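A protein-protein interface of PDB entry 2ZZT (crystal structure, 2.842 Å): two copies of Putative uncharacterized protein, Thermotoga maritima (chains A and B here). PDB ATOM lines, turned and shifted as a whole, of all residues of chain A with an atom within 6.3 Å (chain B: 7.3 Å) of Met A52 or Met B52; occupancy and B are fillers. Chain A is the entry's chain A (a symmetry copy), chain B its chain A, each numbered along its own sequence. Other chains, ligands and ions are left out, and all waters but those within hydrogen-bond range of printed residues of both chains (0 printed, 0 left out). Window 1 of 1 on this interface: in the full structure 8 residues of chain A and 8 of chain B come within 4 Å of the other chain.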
ATOM      1  N   ASN A  24      -9.798 -26.588  -7.419  1.00  0.00           N
ATOM      2  CA  ASN A  24     -10.493 -25.700  -8.325  1.00  0.00           C
ATOM      3  C   ASN A  24     -12.007 -25.932  -8.315  1.00  0.00           C
ATOM      4  O   ASN A  24     -12.759 -25.122  -8.842  1.00  0.00           O
ATOM      5  CB  ASN A  24      -9.911 -25.825  -9.744  1.00  0.00           C
ATOM      6  CG  ASN A  24      -9.216 -27.160  -9.979  1.00  0.00           C
ATOM      7  OD1 ASN A  24      -9.436 -28.139  -9.250  1.00  0.00           O
ATOM      8  ND2 ASN A  24      -8.383 -27.212 -11.007  1.00  0.00           N
ATOM      9  N   VAL A  25     -12.454 -27.016  -7.684  1.00  0.00           N
ATOM     10  CA  VAL A  25     -13.883 -27.364  -7.669  1.00  0.00           C
ATOM     11  C   VAL A  25     -14.637 -26.760  -6.453  1.00  0.00           C
ATOM     12  O   VAL A  25     -14.106 -26.768  -5.335  1.00  0.00           O
ATOM     13  CB  VAL A  25     -14.061 -28.885  -7.785  1.00  0.00           C
ATOM     14  CG1 VAL A  25     -15.535 -29.262  -7.845  1.00  0.00           C
ATOM     15  CG2 VAL A  25     -13.350 -29.377  -9.032  1.00  0.00           C
ATOM     16  N   VAL A  48     -17.163 -23.407 -11.153  1.00  0.00           N
ATOM     17  CA  VAL A  48     -15.763 -23.029 -11.322  1.00  0.00           C
ATOM     18  C   VAL A  48     -15.593 -21.582 -11.749  1.00  0.00           C
ATOM     19  O   VAL A  48     -16.571 -20.919 -12.095  1.00  0.00           O
ATOM     20  CB  VAL A  48     -14.985 -23.963 -12.257  1.00  0.00           C
ATOM     21  CG1 VAL A  48     -15.635 -25.317 -12.321  1.00  0.00           C
ATOM     22  CG2 VAL A  48     -14.847 -23.369 -13.633  1.00  0.00           C
ATOM     23  N   ASP A  49     -14.346 -21.111 -11.700  1.00  0.00           N
ATOM     24  CA  ASP A  49     -13.941 -19.751 -12.088  1.00  0.00           C
ATOM     25  C   ASP A  49     -14.499 -19.313 -13.431  1.00  0.00           C
ATOM     26  O   ASP A  49     -14.021 -19.773 -14.472  1.00  0.00           O
ATOM     27  CB  ASP A  49     -12.408 -19.691 -12.182  1.00  0.00           C
ATOM     28  CG  ASP A  49     -11.860 -18.280 -12.075  1.00  0.00           C
ATOM     29  OD1 ASP A  49     -10.785 -18.009 -12.672  1.00  0.00           O
ATOM     30  OD2 ASP A  49     -12.504 -17.455 -11.391  1.00  0.00           O
ATOM     31  N   GLY A  50     -15.497 -18.432 -13.408  1.00  0.00           N
ATOM     32  CA  GLY A  50     -15.933 -17.775 -14.625  1.00  0.00           C
ATOM     33  C   GLY A  50     -14.756 -17.677 -15.578  1.00  0.00           C
ATOM     34  O   GLY A  50     -14.833 -18.142 -16.717  1.00  0.00           O
ATOM     35  N   LYS A  51     -13.645 -17.117 -15.109  1.00  0.00           N
ATOM     36  CA  LYS A  51     -12.464 -17.021 -15.956  1.00  0.00           C
ATOM     37  C   LYS A  51     -11.810 -18.354 -16.343  1.00  0.00           C
ATOM     38  O   LYS A  51     -10.742 -18.352 -16.943  1.00  0.00           O
ATOM     39  CB  LYS A  51     -11.403 -16.095 -15.343  1.00  0.00           C
ATOM     40  CG  LYS A  51     -11.881 -14.704 -14.941  1.00  0.00           C
ATOM     41  CD  LYS A  51     -10.806 -13.656 -15.218  1.00  0.00           C
ATOM     42  CE  LYS A  51     -10.699 -13.390 -16.712  1.00  0.00           C
ATOM     43  NZ  LYS A  51      -9.293 -13.324 -17.197  1.00  0.00           N
ATOM     44  N   MET A  52     -12.410 -19.492 -16.023  1.00  0.00           N
ATOM     45  CA  MET A  52     -11.750 -20.730 -16.408  1.00  0.00           C
ATOM     46  C   MET A  52     -12.064 -21.053 -17.854  1.00  0.00           C
ATOM     47  O   MET A  52     -13.134 -20.736 -18.376  1.00  0.00           O
ATOM     48  CB  MET A  52     -12.092 -21.916 -15.507  1.00  0.00           C
ATOM     49  CG  MET A  52     -11.343 -23.194 -15.905  1.00  0.00           C
ATOM     50  SD  MET A  52     -11.723 -24.882 -14.927  1.00  0.00           S
ATOM     51  CE  MET A  52     -11.599 -24.238 -13.113  1.00  0.00           C
ATOM     52  N   SER A  53     -11.097 -21.669 -18.504  1.00  0.00           N
ATOM     53  CA  SER A  53     -11.257 -22.006 -19.882  1.00  0.00           C
ATOM     54  C   SER A  53     -12.093 -23.258 -19.990  1.00  0.00           C
ATOM     55  O   SER A  53     -11.885 -24.265 -19.299  1.00  0.00           O
ATOM     56  CB  SER A  53      -9.909 -22.254 -20.539  1.00  0.00           C
ATOM     57  OG  SER A  53      -9.638 -23.645 -20.588  1.00  0.00           O
ATOM     58  N   VAL A  54     -13.055 -23.171 -20.883  1.00  0.00           N
ATOM     59  CA  VAL A  54     -13.867 -24.292 -21.240  1.00  0.00           C
ATOM     60  C   VAL A  54     -13.015 -25.555 -21.429  1.00  0.00           C
ATOM     61  O   VAL A  54     -13.356 -26.622 -20.936  1.00  0.00           O
ATOM     62  CB  VAL A  54     -14.665 -23.900 -22.474  1.00  0.00           C
ATOM     63  CG1 VAL A  54     -15.230 -25.109 -23.202  1.00  0.00           C
ATOM     64  CG2 VAL A  54     -15.764 -22.922 -22.071  1.00  0.00           C
ATOM     65  N   LYS A  55     -11.894 -25.438 -22.115  1.00  0.00           N
ATOM     66  CA  LYS A  55     -11.094 -26.620 -22.368  1.00  0.00           C
ATOM     67  C   LYS A  55     -10.571 -27.180 -21.071  1.00  0.00           C
ATOM     68  O   LYS A  55     -10.364 -28.386 -20.933  1.00  0.00           O
ATOM     69  CB  LYS A  55      -9.912 -26.304 -23.258  1.00  0.00           C
ATOM     70  CG  LYS A  55      -8.759 -27.232 -22.968  1.00  0.00           C
ATOM     71  CD  LYS A  55      -7.542 -26.922 -23.810  1.00  0.00           C
ATOM     72  CE  LYS A  55      -6.264 -27.172 -23.019  1.00  0.00           C
ATOM     73  NZ  LYS A  55      -5.119 -27.559 -23.898  1.00  0.00           N
ATOM     74  N   ASP A  56     -10.341 -26.305 -20.111  1.00  0.00           N
ATOM     75  CA  ASP A  56      -9.797 -26.775 -18.869  1.00  0.00           C
ATOM     76  C   ASP A  56     -10.890 -27.477 -18.153  1.00  0.00           C
ATOM     77  O   ASP A  56     -10.784 -28.637 -17.780  1.00  0.00           O
ATOM     78  CB  ASP A  56      -9.320 -25.605 -18.039  1.00  0.00           C
ATOM     79  CG  ASP A  56      -7.954 -25.148 -18.445  1.00  0.00           C
ATOM     80  OD1 ASP A  56      -7.175 -26.005 -18.914  1.00  0.00           O
ATOM     81  OD2 ASP A  56      -7.666 -23.939 -18.309  1.00  0.00           O
ATOM     82  N   ALA A  57     -11.967 -26.747 -17.968  1.00  0.00           N
ATOM     83  CA  ALA A  57     -13.088 -27.304 -17.290  1.00  0.00           C
ATOM     84  C   ALA A  57     -13.383 -28.628 -17.941  1.00  0.00           C
ATOM     85  O   ALA A  57     -13.732 -29.572 -17.270  1.00  0.00           O
ATOM     86  CB  ALA A  57     -14.243 -26.394 -17.367  1.00  0.00           C
ATOM     87  N   HIS A  58     -13.231 -28.753 -19.244  1.00  0.00           N
ATOM     88  CA  HIS A  58     -13.526 -30.069 -19.774  1.00  0.00           C
ATOM     89  C   HIS A  58     -12.615 -31.056 -19.075  1.00  0.00           C
ATOM     90  O   HIS A  58     -13.067 -31.956 -18.370  1.00  0.00           O
ATOM     91  CB  HIS A  58     -13.333 -30.171 -21.280  1.00  0.00           C
ATOM     92  CG  HIS A  58     -13.527 -31.562 -21.794  1.00  0.00           C
ATOM     93  ND1 HIS A  58     -14.755 -32.192 -21.784  1.00  0.00           N
ATOM     94  CD2 HIS A  58     -12.651 -32.459 -22.299  1.00  0.00           C
ATOM     95  CE1 HIS A  58     -14.628 -33.410 -22.275  1.00  0.00           C
ATOM     96  NE2 HIS A  58     -13.360 -33.598 -22.594  1.00  0.00           N
ATOM     97  N   LEU A  60     -11.128 -31.014 -16.501  1.00  0.00           N
ATOM     98  CA  LEU A  60     -11.412 -31.183 -15.090  1.00  0.00           C
ATOM     99  C   LEU A  60     -12.410 -32.290 -14.845  1.00  0.00           C
ATOM    100  O   LEU A  60     -12.138 -33.210 -14.088  1.00  0.00           O
ATOM    101  CB  LEU A  60     -11.894 -29.870 -14.468  1.00  0.00           C
ATOM    102  CG  LEU A  60     -12.304 -29.851 -12.989  1.00  0.00           C
ATOM    103  CD1 LEU A  60     -11.223 -30.390 -12.075  1.00  0.00           C
ATOM    104  CD2 LEU A  60     -12.690 -28.457 -12.547  1.00  0.00           C
ATOM    105  N   ASN B  24     -20.491 -17.990 -32.568  1.00  0.00           N
ATOM    106  CA  ASN B  24     -19.566 -18.671 -31.689  1.00  0.00           C
ATOM    107  C   ASN B  24     -19.948 -20.140 -31.474  1.00  0.00           C
ATOM    108  O   ASN B  24     -19.156 -20.912 -30.952  1.00  0.00           O
ATOM    109  CB  ASN B  24     -19.446 -17.917 -30.354  1.00  0.00           C
ATOM    110  CG  ASN B  24     -20.663 -17.050 -30.057  1.00  0.00           C
ATOM    111  OD1 ASN B  24     -21.745 -17.238 -30.631  1.00  0.00           O
ATOM    112  ND2 ASN B  24     -20.495 -16.102 -29.147  1.00  0.00           N
ATOM    113  N   VAL B  25     -21.145 -20.529 -31.911  1.00  0.00           N
ATOM    114  CA  VAL B  25     -21.633 -21.899 -31.698  1.00  0.00           C
ATOM    115  C   VAL B  25     -21.272 -22.856 -32.867  1.00  0.00           C
ATOM    116  O   VAL B  25     -21.372 -22.462 -34.036  1.00  0.00           O
ATOM    117  CB  VAL B  25     -23.136 -21.885 -31.383  1.00  0.00           C
ATOM    118  CG1 VAL B  25     -23.648 -23.289 -31.087  1.00  0.00           C
ATOM    119  CG2 VAL B  25     -23.387 -20.981 -30.190  1.00  0.00           C
ATOM    120  N   HIS B  26     -20.853 -24.094 -32.560  1.00  0.00           N
ATOM    121  CA  HIS B  26     -20.313 -25.016 -33.571  1.00  0.00           C
ATOM    122  C   HIS B  26     -20.696 -26.448 -33.314  1.00  0.00           C
ATOM    123  O   HIS B  26     -21.018 -26.821 -32.206  1.00  0.00           O
ATOM    124  CB  HIS B  26     -18.777 -24.959 -33.617  1.00  0.00           C
ATOM    125  CG  HIS B  26     -18.231 -23.657 -34.111  1.00  0.00           C
ATOM    126  ND1 HIS B  26     -18.145 -23.339 -35.449  1.00  0.00           N
ATOM    127  CD2 HIS B  26     -17.768 -22.573 -33.438  1.00  0.00           C
ATOM    128  CE1 HIS B  26     -17.651 -22.120 -35.582  1.00  0.00           C
ATOM    129  NE2 HIS B  26     -17.418 -21.635 -34.375  1.00  0.00           N
ATOM    130  N   GLU B  47     -20.337 -27.252 -29.357  1.00  0.00           N
ATOM    131  CA  GLU B  47     -18.905 -27.041 -29.126  1.00  0.00           C
ATOM    132  C   GLU B  47     -18.532 -25.587 -29.166  1.00  0.00           C
ATOM    133  O   GLU B  47     -19.065 -24.837 -29.955  1.00  0.00           O
ATOM    134  CB  GLU B  47     -18.076 -27.777 -30.154  1.00  0.00           C
ATOM    135  CG  GLU B  47     -17.949 -29.234 -29.802  1.00  0.00           C
ATOM    136  CD  GLU B  47     -17.606 -30.073 -30.982  1.00  0.00           C
ATOM    137  OE1 GLU B  47     -17.376 -29.473 -32.041  1.00  0.00           O
ATOM    138  OE2 GLU B  47     -17.568 -31.315 -30.868  1.00  0.00           O
ATOM    139  N   VAL B  48     -17.604 -25.185 -28.303  1.00  0.00           N
ATOM    140  CA  VAL B  48     -17.068 -23.828 -28.364  1.00  0.00           C
ATOM    141  C   VAL B  48     -15.569 -23.778 -28.134  1.00  0.00           C
ATOM    142  O   VAL B  48     -14.967 -24.778 -27.744  1.00  0.00           O
ATOM    143  CB  VAL B  48     -17.790 -22.844 -27.434  1.00  0.00           C
ATOM    144  CG1 VAL B  48     -19.183 -23.321 -27.129  1.00  0.00           C
ATOM    145  CG2 VAL B  48     -17.010 -22.615 -26.168  1.00  0.00           C
ATOM    146  N   ASP B  49     -14.985 -22.608 -28.400  1.00  0.00           N
ATOM    147  CA  ASP B  49     -13.553 -22.321 -28.230  1.00  0.00           C
ATOM    148  C   ASP B  49     -13.001 -22.764 -26.887  1.00  0.00           C
ATOM    149  O   ASP B  49     -13.271 -22.118 -25.870  1.00  0.00           O
ATOM    150  CB  ASP B  49     -13.327 -20.804 -28.345  1.00  0.00           C
ATOM    151  CG  ASP B  49     -11.895 -20.440 -28.687  1.00  0.00           C
ATOM    152  OD1 ASP B  49     -11.441 -19.341 -28.272  1.00  0.00           O
ATOM    153  OD2 ASP B  49     -11.235 -21.250 -29.374  1.00  0.00           O
ATOM    154  N   GLY B  50     -12.235 -23.854 -26.882  1.00  0.00           N
ATOM    155  CA  GLY B  50     -11.472 -24.217 -25.704  1.00  0.00           C
ATOM    156  C   GLY B  50     -11.133 -22.956 -24.931  1.00  0.00           C
ATOM    157  O   GLY B  50     -11.451 -22.845 -23.746  1.00  0.00           O
ATOM    158  N   LYS B  51     -10.531 -21.980 -25.604  1.00  0.00           N
ATOM    159  CA  LYS B  51     -10.207 -20.727 -24.935  1.00  0.00           C
ATOM    160  C   LYS B  51     -11.405 -19.883 -24.483  1.00  0.00           C
ATOM    161  O   LYS B  51     -11.218 -18.759 -24.033  1.00  0.00           O
ATOM    162  CB  LYS B  51      -9.267 -19.859 -25.785  1.00  0.00           C
ATOM    163  CG  LYS B  51      -7.995 -20.539 -26.281  1.00  0.00           C
ATOM    164  CD  LYS B  51      -6.818 -19.568 -26.272  1.00  0.00           C
ATOM    165  CE  LYS B  51      -6.351 -19.318 -24.846  1.00  0.00           C
ATOM    166  NZ  LYS B  51      -6.080 -17.881 -24.559  1.00  0.00           N
ATOM    167  N   MET B  52     -12.631 -20.380 -24.587  1.00  0.00           N
ATOM    168  CA  MET B  52     -13.736 -19.541 -24.150  1.00  0.00           C
ATOM    169  C   MET B  52     -13.896 -19.643 -22.646  1.00  0.00           C
ATOM    170  O   MET B  52     -13.623 -20.675 -22.030  1.00  0.00           O
ATOM    171  CB  MET B  52     -15.057 -19.846 -24.853  1.00  0.00           C
ATOM    172  CG  MET B  52     -16.190 -18.913 -24.409  1.00  0.00           C
ATOM    173  SD  MET B  52     -18.020 -19.207 -25.125  1.00  0.00           S
ATOM    174  CE  MET B  52     -17.610 -19.371 -27.002  1.00  0.00           C
ATOM    175  N   SER B  53     -14.322 -18.542 -22.060  1.00  0.00           N
ATOM    176  CA  SER B  53     -14.491 -18.500 -20.644  1.00  0.00           C
ATOM    177  C   SER B  53     -15.795 -19.167 -20.281  1.00  0.00           C
ATOM    178  O   SER B  53     -16.857 -18.927 -20.871  1.00  0.00           O
ATOM    179  CB  SER B  53     -14.515 -17.064 -20.145  1.00  0.00           C
ATOM    180  OG  SER B  53     -15.852 -16.631 -19.969  1.00  0.00           O
ATOM    181  N   VAL B  54     -15.689 -20.021 -19.287  1.00  0.00           N
ATOM    182  CA  VAL B  54     -16.829 -20.651 -18.699  1.00  0.00           C
ATOM    183  C   VAL B  54     -17.966 -19.643 -18.476  1.00  0.00           C
ATOM    184  O   VAL B  54     -19.117 -19.912 -18.792  1.00  0.00           O
ATOM    185  CB  VAL B  54     -16.363 -21.340 -17.425  1.00  0.00           C
ATOM    186  CG1 VAL B  54     -17.517 -21.672 -16.494  1.00  0.00           C
ATOM    187  CG2 VAL B  54     -15.561 -22.584 -17.793  1.00  0.00           C
ATOM    188  N   LYS B  55     -17.648 -18.470 -17.960  1.00  0.00           N
ATOM    189  CA  LYS B  55     -18.700 -17.514 -17.677  1.00  0.00           C
ATOM    190  C   LYS B  55     -19.370 -17.085 -18.957  1.00  0.00           C
ATOM    191  O   LYS B  55     -20.557 -16.758 -18.979  1.00  0.00           O
ATOM    192  CB  LYS B  55     -18.155 -16.281 -16.993  1.00  0.00           C
ATOM    193  CG  LYS B  55     -18.992 -15.070 -17.320  1.00  0.00           C
ATOM    194  CD  LYS B  55     -18.454 -13.807 -16.686  1.00  0.00           C
ATOM    195  CE  LYS B  55     -18.676 -12.610 -17.603  1.00  0.00           C
ATOM    196  NZ  LYS B  55     -18.828 -11.333 -16.841  1.00  0.00           N
ATOM    197  N   ASP B  56     -18.610 -17.072 -20.035  1.00  0.00           N
ATOM    198  CA  ASP B  56     -19.180 -16.626 -21.273  1.00  0.00           C
ATOM    199  C   ASP B  56     -20.076 -17.708 -21.754  1.00  0.00           C
ATOM    200  O   ASP B  56     -21.259 -17.512 -22.000  1.00  0.00           O
ATOM    201  CB  ASP B  56     -18.088 -16.389 -22.290  1.00  0.00           C
ATOM    202  CG  ASP B  56     -17.446 -15.046 -22.123  1.00  0.00           C
ATOM    203  OD1 ASP B  56     -18.152 -14.125 -21.662  1.00  0.00           O
ATOM    204  OD2 ASP B  56     -16.242 -14.918 -22.434  1.00  0.00           O
ATOM    205  N   ALA B  57     -19.487 -18.876 -21.880  1.00  0.00           N
ATOM    206  CA  ALA B  57     -20.238 -19.996 -22.337  1.00  0.00           C
ATOM    207  C   ALA B  57     -21.489 -20.058 -21.502  1.00  0.00           C
ATOM    208  O   ALA B  57     -22.542 -20.372 -22.007  1.00  0.00           O
ATOM    209  CB  ALA B  57     -19.447 -21.232 -22.217  1.00  0.00           C
ATOM    210  N   HIS B  58     -21.427 -19.742 -20.225  1.00  0.00           N
ATOM    211  CA  HIS B  58     -22.685 -19.817 -19.510  1.00  0.00           C
ATOM    212  C   HIS B  58     -23.659 -18.887 -20.202  1.00  0.00           C
ATOM    213  O   HIS B  58     -24.683 -19.312 -20.731  1.00  0.00           O
ATOM    214  CB  HIS B  58     -22.571 -19.440 -18.041  1.00  0.00           C
ATOM    215  CG  HIS B  58     -23.895 -19.410 -17.347  1.00  0.00           C
ATOM    216  ND1 HIS B  58     -24.639 -20.549 -17.123  1.00  0.00           N
ATOM    217  CD2 HIS B  58     -24.626 -18.383 -16.859  1.00  0.00           C
ATOM    218  CE1 HIS B  58     -25.764 -20.225 -16.513  1.00  0.00           C
ATOM    219  NE2 HIS B  58     -25.782 -18.916 -16.343  1.00  0.00           N
ATOM    220  N   LEU B  60     -23.804 -17.727 -22.935  1.00  0.00           N
ATOM    221  CA  LEU B  60     -24.183 -18.153 -24.267  1.00  0.00           C
ATOM    222  C   LEU B  60     -25.408 -19.037 -24.249  1.00  0.00           C
ATOM    223  O   LEU B  60     -26.386 -18.750 -24.922  1.00  0.00           O
ATOM    224  CB  LEU B  60     -23.018 -18.852 -24.970  1.00  0.00           C
ATOM    225  CG  LEU B  60     -23.233 -19.432 -26.376  1.00  0.00           C
ATOM    226  CD1 LEU B  60     -23.776 -18.410 -27.353  1.00  0.00           C
ATOM    227  CD2 LEU B  60     -21.955 -20.025 -26.923  1.00  0.00           C
ATOM    228  N   VAL B  82     -21.831 -28.259 -23.185  1.00  0.00           N
ATOM    229  CA  VAL B  82     -20.827 -27.578 -23.986  1.00  0.00           C
ATOM    230  C   VAL B  82     -19.493 -28.288 -23.993  1.00  0.00           C
ATOM    231  O   VAL B  82     -19.060 -28.810 -22.973  1.00  0.00           O
ATOM    232  CB  VAL B  82     -20.625 -26.170 -23.490  1.00  0.00           C
ATOM    233  CG1 VAL B  82     -19.644 -25.458 -24.374  1.00  0.00           C
ATOM    234  CG2 VAL B  82     -21.954 -25.432 -23.482  1.00  0.00           C
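The backbone NH (N) of Val A54 lies within hydrogen-bond range of the backbone carbonyl oxygen (O) of Gly B50 (3.3 Å).
The backbone carbonyl oxygen of Gly B50 lies within hydrogen-bond range of the backbone NH of Lys A55 (3.1 Å).
N of Val A54 is in hydrogen-bond range of O of Met B52 (2.8 Å).
The backbone NH (N) of Val B54 lies within hydrogen-bond range of the backbone carbonyl oxygen (O) of Gly A50, 3.3 Å away.
The backbone NH (N) of Val B54 sits at hydrogen-bond distance from the backbone carbonyl oxygen (O) of Met A52 (2.8 Å).
O of Gly A50 is in hydrogen-bond range of N of Lys B55 (3.1 Å).
The backbone NH (N) of Ala B57 sits at hydrogen-bond distance from the side-chain sulfur (SD) of Met B52 (3.6 Å).
The backbone NH (N) of Lys B55 lies close to the side-chain hydroxyl (OG) of Ser B53, at 3.3 Å.
The backbone NH (N) of Asp B56 is in hydrogen-bond range of the side-chain hydroxyl (OG) of Ser B53.
The side-chain sulfur (SD) of Met A52 lies within hydrogen-bond range of the backbone NH (N) of Ala A57.
The backbone NH of Lys A55 sits close to the side-chain hydroxyl of Ser A53, at 3.3 Å.
OG of Ser A53 is in hydrogen-bond range of N of Asp A56.
Among the printed residues, pairs that only touch across the chains: Gly A50 with Ser B53 (3.6 Å), Met A52 with Met B52 (3.7 Å), Met A52 with Ser B53 (3.5 Å), Ser A53 with Gly B50 (3.6 Å) and Ser A53 with Met B52 (3.5 Å).
Of the printed residues of chain B, Met A52 touches Met B52 (3.7 Å), Ser B53 (3.5 Å) and Val B54 (2.8 Å).
Printed residues of chain B within 4 Å of Ser A53: Gly B50 (3.6 Å) and Met B52 (3.5 Å).
Printed residues of chain A within 4 Å of Ser B53: Gly A50 and Met A52.
Of the printed residues of chain A, Gly B50 touches Ser A53 (3.6 Å), Val A54 (3.3 Å) and Lys A55 (3.1 Å).
Asp B49 touches none of the printed residues of chain A.
The nearest residue of chain B that does not touch Met A52 is Lys B55 (5.1 Å).
The nearest residue of chain A that does not touch Met B52 is Lys A55 (5.1 Å).
The nearest printed residue of chain A that does not touch Gly B50 is Asp A56 (5.1 Å).
Hydrophobic or aromatic side chains of chain A that line the printed part of chain B: Val A54.
Printed residues of chain B that touch a printed residue of chain A: Gly B50, Met B52, Ser B53, Val B54 and Lys B55.
Hydrophobic or aromatic side chains of chain B within 4 Å of the printed part of chain A: Val B54.
Among the printed residues, 11 pairs touch across the chains.
Among the printed residues, no Asp or Glu carboxylate lies within 4 Å of a Lys or Arg side-chain nitrogen of the other chain.
Gly A50 touches Ser B53, and with the chains exchanged Ser A53 touches Gly B50.
Gly A50 touches Lys B55, and with the chains exchanged Lys A55 touches Gly B50.
Met B52 touches its own counterpart, Met A52.
Met A52 touches Ser B53, and with the chains exchanged Ser A53 touches Met B52.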
